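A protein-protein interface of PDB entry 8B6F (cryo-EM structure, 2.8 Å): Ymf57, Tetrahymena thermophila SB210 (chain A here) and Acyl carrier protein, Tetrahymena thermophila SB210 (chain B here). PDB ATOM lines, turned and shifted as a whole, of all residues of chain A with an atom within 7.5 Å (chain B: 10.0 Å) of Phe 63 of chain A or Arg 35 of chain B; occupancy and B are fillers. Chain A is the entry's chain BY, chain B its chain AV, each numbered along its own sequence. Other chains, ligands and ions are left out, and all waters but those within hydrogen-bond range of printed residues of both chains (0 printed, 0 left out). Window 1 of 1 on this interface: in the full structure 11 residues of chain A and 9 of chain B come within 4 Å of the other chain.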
ATOM      1  N   THR A  57     -35.024  -6.449  22.164  1.00  0.00           N
ATOM      2  CA  THR A  57     -34.753  -5.026  22.002  1.00  0.00           C
ATOM      3  C   THR A  57     -33.621  -4.582  22.921  1.00  0.00           C
ATOM      4  O   THR A  57     -32.666  -3.933  22.480  1.00  0.00           O
ATOM      5  CB  THR A  57     -36.022  -4.218  22.284  1.00  0.00           C
ATOM      6  OG1 THR A  57     -37.063  -4.626  21.388  1.00  0.00           O
ATOM      7  CG2 THR A  57     -35.766  -2.733  22.101  1.00  0.00           C
ATOM      8  N   ILE A  58     -33.720  -4.911  24.208  1.00  0.00           N
ATOM      9  CA  ILE A  58     -32.686  -4.506  25.153  1.00  0.00           C
ATOM     10  C   ILE A  58     -31.385  -5.247  24.873  1.00  0.00           C
ATOM     11  O   ILE A  58     -30.294  -4.674  24.973  1.00  0.00           O
ATOM     12  CB  ILE A  58     -33.176  -4.733  26.593  1.00  0.00           C
ATOM     13  CG1 ILE A  58     -34.437  -3.909  26.850  1.00  0.00           C
ATOM     14  CG2 ILE A  58     -32.091  -4.370  27.596  1.00  0.00           C
ATOM     15  CD1 ILE A  58     -35.234  -4.376  28.033  1.00  0.00           C
ATOM     16  N   ASP A  59     -31.475  -6.530  24.522  1.00  0.00           N
ATOM     17  CA  ASP A  59     -30.273  -7.298  24.216  1.00  0.00           C
ATOM     18  C   ASP A  59     -29.532  -6.704  23.026  1.00  0.00           C
ATOM     19  O   ASP A  59     -28.305  -6.561  23.056  1.00  0.00           O
ATOM     20  CB  ASP A  59     -30.637  -8.758  23.948  1.00  0.00           C
ATOM     21  CG  ASP A  59     -29.424  -9.609  23.628  1.00  0.00           C
ATOM     22  OD1 ASP A  59     -28.553  -9.760  24.510  1.00  0.00           O
ATOM     23  OD2 ASP A  59     -29.341 -10.127  22.494  1.00  0.00           O
ATOM     24  N   SER A  60     -30.264  -6.351  21.968  1.00  0.00           N
ATOM     25  CA  SER A  60     -29.633  -5.756  20.796  1.00  0.00           C
ATOM     26  C   SER A  60     -29.071  -4.377  21.112  1.00  0.00           C
ATOM     27  O   SER A  60     -28.010  -4.003  20.601  1.00  0.00           O
ATOM     28  CB  SER A  60     -30.635  -5.676  19.645  1.00  0.00           C
ATOM     29  OG  SER A  60     -31.727  -4.835  19.972  1.00  0.00           O
ATOM     30  N   PHE A  61     -29.768  -3.603  21.947  1.00  0.00           N
ATOM     31  CA  PHE A  61     -29.233  -2.313  22.368  1.00  0.00           C
ATOM     32  C   PHE A  61     -27.891  -2.488  23.066  1.00  0.00           C
ATOM     33  O   PHE A  61     -26.927  -1.771  22.776  1.00  0.00           O
ATOM     34  CB  PHE A  61     -30.232  -1.613  23.289  1.00  0.00           C
ATOM     35  CG  PHE A  61     -29.759  -0.281  23.796  1.00  0.00           C
ATOM     36  CD1 PHE A  61     -29.903   0.857  23.020  1.00  0.00           C
ATOM     37  CD2 PHE A  61     -29.178  -0.165  25.047  1.00  0.00           C
ATOM     38  CE1 PHE A  61     -29.473   2.085  23.479  1.00  0.00           C
ATOM     39  CE2 PHE A  61     -28.745   1.061  25.513  1.00  0.00           C
ATOM     40  CZ  PHE A  61     -28.892   2.188  24.727  1.00  0.00           C
ATOM     41  N   ILE A  62     -27.813  -3.440  23.997  1.00  0.00           N
ATOM     42  CA  ILE A  62     -26.568  -3.669  24.724  1.00  0.00           C
ATOM     43  C   ILE A  62     -25.467  -4.108  23.767  1.00  0.00           C
ATOM     44  O   ILE A  62     -24.331  -3.627  23.842  1.00  0.00           O
ATOM     45  CB  ILE A  62     -26.797  -4.697  25.847  1.00  0.00           C
ATOM     46  CG1 ILE A  62     -27.729  -4.112  26.911  1.00  0.00           C
ATOM     47  CG2 ILE A  62     -25.476  -5.122  26.473  1.00  0.00           C
ATOM     48  CD1 ILE A  62     -28.211  -5.120  27.934  1.00  0.00           C
ATOM     49  N   PHE A  63     -25.783  -5.030  22.856  1.00  0.00           N
ATOM     50  CA  PHE A  63     -24.779  -5.532  21.925  1.00  0.00           C
ATOM     51  C   PHE A  63     -24.271  -4.422  21.012  1.00  0.00           C
ATOM     52  O   PHE A  63     -23.063  -4.285  20.796  1.00  0.00           O
ATOM     53  CB  PHE A  63     -25.361  -6.682  21.104  1.00  0.00           C
ATOM     54  CG  PHE A  63     -24.326  -7.508  20.398  1.00  0.00           C
ATOM     55  CD1 PHE A  63     -23.720  -8.575  21.040  1.00  0.00           C
ATOM     56  CD2 PHE A  63     -23.965  -7.228  19.091  1.00  0.00           C
ATOM     57  CE1 PHE A  63     -22.770  -9.341  20.396  1.00  0.00           C
ATOM     58  CE2 PHE A  63     -23.016  -7.991  18.441  1.00  0.00           C
ATOM     59  CZ  PHE A  63     -22.417  -9.048  19.095  1.00  0.00           C
ATOM     60  N   ASN A  64     -25.184  -3.615  20.470  1.00  0.00           N
ATOM     61  CA  ASN A  64     -24.783  -2.539  19.569  1.00  0.00           C
ATOM     62  C   ASN A  64     -23.957  -1.485  20.297  1.00  0.00           C
ATOM     63  O   ASN A  64     -23.001  -0.943  19.735  1.00  0.00           O
ATOM     64  CB  ASN A  64     -26.015  -1.906  18.926  1.00  0.00           C
ATOM     65  CG  ASN A  64     -26.822  -2.900  18.115  1.00  0.00           C
ATOM     66  OD1 ASN A  64     -26.284  -3.870  17.587  1.00  0.00           O
ATOM     67  ND2 ASN A  64     -28.122  -2.657  18.005  1.00  0.00           N
ATOM     68  N   ASN A  65     -24.318  -1.169  21.540  1.00  0.00           N
ATOM     69  CA  ASN A  65     -23.512  -0.237  22.323  1.00  0.00           C
ATOM     70  C   ASN A  65     -22.126  -0.806  22.593  1.00  0.00           C
ATOM     71  O   ASN A  65     -21.121  -0.097  22.467  1.00  0.00           O
ATOM     72  CB  ASN A  65     -24.215   0.097  23.636  1.00  0.00           C
ATOM     73  CG  ASN A  65     -25.333   1.097  23.456  1.00  0.00           C
ATOM     74  OD1 ASN A  65     -25.193   2.267  23.807  1.00  0.00           O
ATOM     75  ND2 ASN A  65     -26.448   0.646  22.900  1.00  0.00           N
ATOM     76  N   ASN A  66     -22.050  -2.086  22.957  1.00  0.00           N
ATOM     77  CA  ASN A  66     -20.760  -2.711  23.213  1.00  0.00           C
ATOM     78  C   ASN A  66     -19.904  -2.792  21.958  1.00  0.00           C
ATOM     79  O   ASN A  66     -18.678  -2.901  22.070  1.00  0.00           O
ATOM     80  CB  ASN A  66     -20.960  -4.115  23.786  1.00  0.00           C
ATOM     81  CG  ASN A  66     -21.636  -4.107  25.145  1.00  0.00           C
ATOM     82  OD1 ASN A  66     -22.368  -5.036  25.485  1.00  0.00           O
ATOM     83  ND2 ASN A  66     -21.381  -3.075  25.938  1.00  0.00           N
ATOM     84  N   ARG A  67     -20.513  -2.751  20.774  1.00  0.00           N
ATOM     85  CA  ARG A  67     -19.722  -2.696  19.549  1.00  0.00           C
ATOM     86  C   ARG A  67     -18.757  -1.521  19.568  1.00  0.00           C
ATOM     87  O   ARG A  67     -17.689  -1.585  18.951  1.00  0.00           O
ATOM     88  CB  ARG A  67     -20.633  -2.592  18.328  1.00  0.00           C
ATOM     89  CG  ARG A  67     -21.349  -3.875  17.953  1.00  0.00           C
ATOM     90  CD  ARG A  67     -22.183  -3.669  16.699  1.00  0.00           C
ATOM     91  NE  ARG A  67     -22.863  -4.888  16.278  1.00  0.00           N
ATOM     92  CZ  ARG A  67     -22.338  -5.810  15.483  1.00  0.00           C
ATOM     93  NH1 ARG A  67     -21.108  -5.700  15.013  1.00  0.00           N
ATOM     94  NH2 ARG A  67     -23.070  -6.868  15.148  1.00  0.00           N
ATOM     95  N   PHE A  68     -19.114  -0.439  20.261  1.00  0.00           N
ATOM     96  CA  PHE A  68     -18.318   0.779  20.274  1.00  0.00           C
ATOM     97  C   PHE A  68     -17.505   0.950  21.552  1.00  0.00           C
ATOM     98  O   PHE A  68     -16.958   2.032  21.783  1.00  0.00           O
ATOM     99  CB  PHE A  68     -19.228   1.989  20.068  1.00  0.00           C
ATOM    100  CG  PHE A  68     -19.910   2.005  18.732  1.00  0.00           C
ATOM    101  CD1 PHE A  68     -21.075   1.285  18.527  1.00  0.00           C
ATOM    102  CD2 PHE A  68     -19.386   2.734  17.681  1.00  0.00           C
ATOM    103  CE1 PHE A  68     -21.705   1.292  17.299  1.00  0.00           C
ATOM    104  CE2 PHE A  68     -20.010   2.746  16.450  1.00  0.00           C
ATOM    105  CZ  PHE A  68     -21.170   2.023  16.259  1.00  0.00           C
ATOM    106  N   ASN A  69     -17.413  -0.083  22.384  1.00  0.00           N
ATOM    107  CA  ASN A  69     -16.649  -0.036  23.623  1.00  0.00           C
ATOM    108  C   ASN A  69     -15.430  -0.938  23.501  1.00  0.00           C
ATOM    109  O   ASN A  69     -15.559  -2.116  23.153  1.00  0.00           O
ATOM    110  CB  ASN A  69     -17.503  -0.468  24.819  1.00  0.00           C
ATOM    111  CG  ASN A  69     -18.602   0.525  25.143  1.00  0.00           C
ATOM    112  OD1 ASN A  69     -19.782   0.178  25.164  1.00  0.00           O
ATOM    113  ND2 ASN A  69     -18.218   1.769  25.403  1.00  0.00           N
ATOM    114  N   PHE A  70     -14.252  -0.387  23.784  1.00  0.00           N
ATOM    115  CA  PHE A  70     -13.033  -1.180  23.811  1.00  0.00           C
ATOM    116  C   PHE A  70     -12.995  -2.024  25.077  1.00  0.00           C
ATOM    117  O   PHE A  70     -13.178  -1.507  26.183  1.00  0.00           O
ATOM    118  CB  PHE A  70     -11.800  -0.278  23.743  1.00  0.00           C
ATOM    119  CG  PHE A  70     -11.492   0.225  22.366  1.00  0.00           C
ATOM    120  CD1 PHE A  70     -10.669  -0.499  21.521  1.00  0.00           C
ATOM    121  CD2 PHE A  70     -12.017   1.425  21.918  1.00  0.00           C
ATOM    122  CE1 PHE A  70     -10.382  -0.040  20.253  1.00  0.00           C
ATOM    123  CE2 PHE A  70     -11.732   1.888  20.652  1.00  0.00           C
ATOM    124  CZ  PHE A  70     -10.912   1.154  19.817  1.00  0.00           C
ATOM    125  N   PHE B  27     -32.491  -4.268  16.602  1.00  0.00           N
ATOM    126  CA  PHE B  27     -32.213  -5.650  16.120  1.00  0.00           C
ATOM    127  C   PHE B  27     -30.714  -5.914  16.105  1.00  0.00           C
ATOM    128  O   PHE B  27     -29.933  -5.083  15.648  1.00  0.00           O
ATOM    129  CB  PHE B  27     -32.802  -5.857  14.722  1.00  0.00           C
ATOM    130  CG  PHE B  27     -32.682  -7.264  14.215  1.00  0.00           C
ATOM    131  CD1 PHE B  27     -33.653  -8.202  14.510  1.00  0.00           C
ATOM    132  CD2 PHE B  27     -31.602  -7.644  13.439  1.00  0.00           C
ATOM    133  CE1 PHE B  27     -33.548  -9.496  14.045  1.00  0.00           C
ATOM    134  CE2 PHE B  27     -31.490  -8.937  12.971  1.00  0.00           C
ATOM    135  CZ  PHE B  27     -32.466  -9.864  13.274  1.00  0.00           C
ATOM    136  N   GLN B  28     -30.321  -7.084  16.604  1.00  0.00           N
ATOM    137  CA  GLN B  28     -28.924  -7.493  16.665  1.00  0.00           C
ATOM    138  C   GLN B  28     -28.627  -8.358  15.445  1.00  0.00           C
ATOM    139  O   GLN B  28     -29.065  -9.511  15.372  1.00  0.00           O
ATOM    140  CB  GLN B  28     -28.638  -8.250  17.959  1.00  0.00           C
ATOM    141  CG  GLN B  28     -27.201  -8.709  18.108  1.00  0.00           C
ATOM    142  CD  GLN B  28     -26.985  -9.509  19.371  1.00  0.00           C
ATOM    143  OE1 GLN B  28     -27.807  -9.479  20.285  1.00  0.00           O
ATOM    144  NE2 GLN B  28     -25.880 -10.239  19.428  1.00  0.00           N
ATOM    145  N   ASP B  29     -27.883  -7.802  14.493  1.00  0.00           N
ATOM    146  CA  ASP B  29     -27.528  -8.504  13.266  1.00  0.00           C
ATOM    147  C   ASP B  29     -26.206  -9.229  13.487  1.00  0.00           C
ATOM    148  O   ASP B  29     -25.160  -8.593  13.647  1.00  0.00           O
ATOM    149  CB  ASP B  29     -27.431  -7.523  12.101  1.00  0.00           C
ATOM    150  CG  ASP B  29     -27.121  -8.206  10.787  1.00  0.00           C
ATOM    151  OD1 ASP B  29     -27.144  -9.453  10.744  1.00  0.00           O
ATOM    152  OD2 ASP B  29     -26.848  -7.496   9.798  1.00  0.00           O
ATOM    153  N   ASN B  30     -26.251 -10.562  13.487  1.00  0.00           N
ATOM    154  CA  ASN B  30     -25.059 -11.361  13.729  1.00  0.00           C
ATOM    155  C   ASN B  30     -24.154 -11.464  12.511  1.00  0.00           C
ATOM    156  O   ASN B  30     -23.009 -11.908  12.649  1.00  0.00           O
ATOM    157  CB  ASN B  30     -25.451 -12.768  14.184  1.00  0.00           C
ATOM    158  CG  ASN B  30     -26.161 -12.770  15.522  1.00  0.00           C
ATOM    159  OD1 ASN B  30     -25.994 -11.857  16.328  1.00  0.00           O
ATOM    160  ND2 ASN B  30     -26.958 -13.804  15.765  1.00  0.00           N
ATOM    161  N   GLN B  31     -24.629 -11.073  11.330  1.00  0.00           N
ATOM    162  CA  GLN B  31     -23.786 -11.080  10.144  1.00  0.00           C
ATOM    163  C   GLN B  31     -22.877  -9.862  10.065  1.00  0.00           C
ATOM    164  O   GLN B  31     -21.987  -9.829   9.211  1.00  0.00           O
ATOM    165  CB  GLN B  31     -24.652 -11.154   8.884  1.00  0.00           C
ATOM    166  CG  GLN B  31     -25.560 -12.373   8.832  1.00  0.00           C
ATOM    167  CD  GLN B  31     -24.790 -13.677   8.873  1.00  0.00           C
ATOM    168  OE1 GLN B  31     -23.580 -13.704   8.652  1.00  0.00           O
ATOM    169  NE2 GLN B  31     -25.489 -14.768   9.160  1.00  0.00           N
ATOM    170  N   ASP B  32     -23.078  -8.869  10.928  1.00  0.00           N
ATOM    171  CA  ASP B  32     -22.221  -7.690  11.000  1.00  0.00           C
ATOM    172  C   ASP B  32     -21.252  -7.891  12.159  1.00  0.00           C
ATOM    173  O   ASP B  32     -21.618  -7.730  13.326  1.00  0.00           O
ATOM    174  CB  ASP B  32     -23.055  -6.426  11.180  1.00  0.00           C
ATOM    175  CG  ASP B  32     -22.215  -5.166  11.172  1.00  0.00           C
ATOM    176  OD1 ASP B  32     -20.998  -5.261  10.910  1.00  0.00           O
ATOM    177  OD2 ASP B  32     -22.769  -4.078  11.428  1.00  0.00           O
ATOM    178  N   ARG B  33     -20.013  -8.247  11.834  1.00  0.00           N
ATOM    179  CA  ARG B  33     -18.992  -8.535  12.829  1.00  0.00           C
ATOM    180  C   ARG B  33     -18.115  -7.329  13.139  1.00  0.00           C
ATOM    181  O   ARG B  33     -17.156  -7.458  13.906  1.00  0.00           O
ATOM    182  CB  ARG B  33     -18.116  -9.697  12.353  1.00  0.00           C
ATOM    183  CG  ARG B  33     -18.902 -10.894  11.828  1.00  0.00           C
ATOM    184  CD  ARG B  33     -19.766 -11.517  12.911  1.00  0.00           C
ATOM    185  NE  ARG B  33     -20.516 -12.664  12.415  1.00  0.00           N
ATOM    186  CZ  ARG B  33     -20.045 -13.901  12.345  1.00  0.00           C
ATOM    187  NH1 ARG B  33     -18.811 -14.193  12.718  1.00  0.00           N
ATOM    188  NH2 ARG B  33     -20.832 -14.871  11.888  1.00  0.00           N
ATOM    189  N   SER B  34     -18.420  -6.171  12.562  1.00  0.00           N
ATOM    190  CA  SER B  34     -17.574  -4.996  12.718  1.00  0.00           C
ATOM    191  C   SER B  34     -17.691  -4.416  14.122  1.00  0.00           C
ATOM    192  O   SER B  34     -18.763  -4.422  14.730  1.00  0.00           O
ATOM    193  CB  SER B  34     -17.951  -3.938  11.685  1.00  0.00           C
ATOM    194  OG  SER B  34     -19.303  -3.539  11.838  1.00  0.00           O
ATOM    195  N   ARG B  35     -16.571  -3.917  14.634  1.00  0.00           N
ATOM    196  CA  ARG B  35     -16.534  -3.214  15.908  1.00  0.00           C
ATOM    197  C   ARG B  35     -15.289  -2.336  15.915  1.00  0.00           C
ATOM    198  O   ARG B  35     -14.523  -2.306  14.948  1.00  0.00           O
ATOM    199  CB  ARG B  35     -16.554  -4.193  17.085  1.00  0.00           C
ATOM    200  CG  ARG B  35     -15.445  -5.229  17.052  1.00  0.00           C
ATOM    201  CD  ARG B  35     -15.554  -6.203  18.217  1.00  0.00           C
ATOM    202  NE  ARG B  35     -16.819  -6.930  18.210  1.00  0.00           N
ATOM    203  CZ  ARG B  35     -17.869  -6.645  18.971  1.00  0.00           C
ATOM    204  NH1 ARG B  35     -17.848  -5.648  19.839  1.00  0.00           N
ATOM    205  NH2 ARG B  35     -18.969  -7.385  18.862  1.00  0.00           N
ATOM    206  N   VAL B  36     -15.092  -1.611  17.017  1.00  0.00           N
ATOM    207  CA  VAL B  36     -13.962  -0.687  17.102  1.00  0.00           C
ATOM    208  C   VAL B  36     -12.640  -1.438  17.013  1.00  0.00           C
ATOM    209  O   VAL B  36     -11.665  -0.937  16.440  1.00  0.00           O
ATOM    210  CB  VAL B  36     -14.050   0.153  18.391  1.00  0.00           C
ATOM    211  CG1 VAL B  36     -15.258   1.062  18.341  1.00  0.00           C
ATOM    212  CG2 VAL B  36     -14.089  -0.738  19.625  1.00  0.00           C
ATOM    213  N   GLU B  37     -12.579  -2.644  17.579  1.00  0.00           N
ATOM    214  CA  GLU B  37     -11.338  -3.407  17.546  1.00  0.00           C
ATOM    215  C   GLU B  37     -10.947  -3.841  16.140  1.00  0.00           C
ATOM    216  O   GLU B  37      -9.794  -4.229  15.930  1.00  0.00           O
ATOM    217  CB  GLU B  37     -11.447  -4.646  18.438  1.00  0.00           C
ATOM    218  CG  GLU B  37     -11.578  -4.350  19.923  1.00  0.00           C
ATOM    219  CD  GLU B  37     -12.994  -4.007  20.330  1.00  0.00           C
ATOM    220  OE1 GLU B  37     -13.840  -3.799  19.437  1.00  0.00           O
ATOM    221  OE2 GLU B  37     -13.267  -3.955  21.546  1.00  0.00           O
ATOM    222  N   THR B  38     -11.866  -3.785  15.178  1.00  0.00           N
ATOM    223  CA  THR B  38     -11.614  -4.286  13.834  1.00  0.00           C
ATOM    224  C   THR B  38     -11.231  -3.186  12.853  1.00  0.00           C
ATOM    225  O   THR B  38     -11.151  -3.449  11.650  1.00  0.00           O
ATOM    226  CB  THR B  38     -12.838  -5.038  13.308  1.00  0.00           C
ATOM    227  OG1 THR B  38     -13.966  -4.157  13.271  1.00  0.00           O
ATOM    228  CG2 THR B  38     -13.156  -6.225  14.201  1.00  0.00           C
ATOM    229  N   ASN B  39     -10.999  -1.968  13.332  1.00  0.00           N
ATOM    230  CA  ASN B  39     -10.609  -0.885  12.440  1.00  0.00           C
ATOM    231  C   ASN B  39      -9.295  -1.223  11.748  1.00  0.00           C
ATOM    232  O   ASN B  39      -8.336  -1.659  12.390  1.00  0.00           O
ATOM    233  CB  ASN B  39     -10.476   0.416  13.229  1.00  0.00           C
ATOM    234  CG  ASN B  39     -10.170   1.603  12.345  1.00  0.00           C
ATOM    235  OD1 ASN B  39     -10.461   1.593  11.151  1.00  0.00           O
ATOM    236  ND2 ASN B  39      -9.573   2.634  12.929  1.00  0.00           N
ATOM    237  N   SER B  40      -9.254  -1.019  10.430  1.00  0.00           N
ATOM    238  CA  SER B  40      -8.089  -1.354   9.619  1.00  0.00           C
ATOM    239  C   SER B  40      -7.535  -0.144   8.875  1.00  0.00           C
ATOM    240  O   SER B  40      -6.802  -0.307   7.896  1.00  0.00           O
ATOM    241  CB  SER B  40      -8.434  -2.468   8.628  1.00  0.00           C
ATOM    242  OG  SER B  40      -9.461  -2.061   7.742  1.00  0.00           O
ATOM    243  N   ALA B  41      -7.865   1.065   9.320  1.00  0.00           N
ATOM    244  CA  ALA B  41      -7.405   2.271   8.645  1.00  0.00           C
ATOM    245  C   ALA B  41      -5.991   2.614   9.092  1.00  0.00           C
ATOM    246  O   ALA B  41      -5.707   2.681  10.291  1.00  0.00           O
ATOM    247  CB  ALA B  41      -8.350   3.435   8.939  1.00  0.00           C
ATOM    248  N   LYS B  52      -7.633  -6.000   9.271  1.00  0.00           N
ATOM    249  CA  LYS B  52      -6.606  -5.611  10.228  1.00  0.00           C
ATOM    250  C   LYS B  52      -5.459  -6.611  10.283  1.00  0.00           C
ATOM    251  O   LYS B  52      -4.366  -6.257  10.735  1.00  0.00           O
ATOM    252  CB  LYS B  52      -7.234  -5.454  11.614  1.00  0.00           C
ATOM    253  CG  LYS B  52      -6.276  -5.014  12.706  1.00  0.00           C
ATOM    254  CD  LYS B  52      -7.002  -4.894  14.035  1.00  0.00           C
ATOM    255  CE  LYS B  52      -6.067  -4.457  15.145  1.00  0.00           C
ATOM    256  NZ  LYS B  52      -6.768  -4.382  16.457  1.00  0.00           N
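OD2 of Asp 59 of chain A lies close to OE1 of Gln 28 of chain B. The backbone carbonyl oxygen (O) of Asp 29 of chain B lies within hydrogen-bond range of the guanidinium group (NH2) of Arg 67 of chain A (3.1 Å). O of Asp 32 of chain B lies within hydrogen-bond range of NH2 of Arg 67 of chain A. NH1 of Arg 67 of chain A lies within hydrogen-bond range of O of Ser 34 of chain B (2.7 Å). The backbone NH (N) of Val 36 of chain B sits at hydrogen-bond distance from the backbone carbonyl oxygen (O) of Arg 67 of chain A (3.2 Å). O of Asn 69 of chain A sits close to OE2 of Glu 37 of chain B (3.3 Å).
The side-chain amide nitrogen (NE2) of Gln 28 of chain B lies within hydrogen-bond range of the side-chain amide oxygen (OD1) of Asn 30 of chain B, 3.5 Å away. The side-chain carboxylate (OD1) of Asp 32 of chain B lies within hydrogen-bond range of the side-chain hydroxyl (OG) of Ser 34 of chain B, 2.6 Å away. OG1 of Thr 38 of chain B sits at hydrogen-bond distance from O of Arg 35 of chain B, 2.6 Å away. ND2 of Asn 64 of chain A sits at hydrogen-bond distance from O of Ser 60 of chain A, at 2.9 Å. O of Ile 62 of chain A lies close to OD1 of Asn 66 of chain A (2.9 Å). The side-chain amide oxygen of Asn 69 of chain A sits close to the backbone carbonyl oxygen of Asn 65 of chain A, at 3.0 Å.
Among the printed residues, merely in contact across the chains: Phe 63 of chain A with Gln 28 of chain B, Ser 60 of chain A with Gln 28 of chain B, Arg 67 of chain A with Arg 35 of chain B, Ser 60 of chain A with Phe 27 of chain B, Phe 70 of chain A with Val 36 of chain B, Phe 70 of chain A with Glu 37 of chain B, Phe 68 of chain A with Val 36 of chain B, Asn 66 of chain A with Arg 35 of chain B, Phe 63 of chain A with Arg 35 of chain B, Asn 64 of chain A with Phe 27 of chain B and Arg 67 of chain A with Arg 33 of chain B.
Thr 57 of chain A touches none of the printed residues of chain B. Ile 62 of chain A touches none of the printed residues of chain B. Of the printed residues of chain B, Phe 63 of chain A touches Gln 28 and Arg 35. Asn 64 of chain A touches just one residue of chain B: Phe 27. Of the printed residues of chain A, Ser 34 of chain B touches Arg 67. Of chain A, only Phe 63 (3.8 Å), Asn 66 (3.6 Å) and Arg 67 (3.4 Å) come within 4 Å of Arg 35 of chain B. Of the printed residues of chain A, Glu 37 of chain B touches Asn 69 and Phe 70. The nearest printed residue of chain A that does not touch Arg 35 of chain B is Asn 69 of chain A (5.4 Å). The nearest printed residue of chain B that does not touch Phe 68 of chain A is Arg 35 of chain B (5.4 Å).
Of the 16 printed residues of chain B, 9 touch a printed residue of chain A. Hydrophobic or aromatic side chains of chain B within 4 Å of the printed part of chain A: Val 36. Hydrophobic or aromatic side chains of chain A that line the printed part of chain B: Phe 63 and Phe 70.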
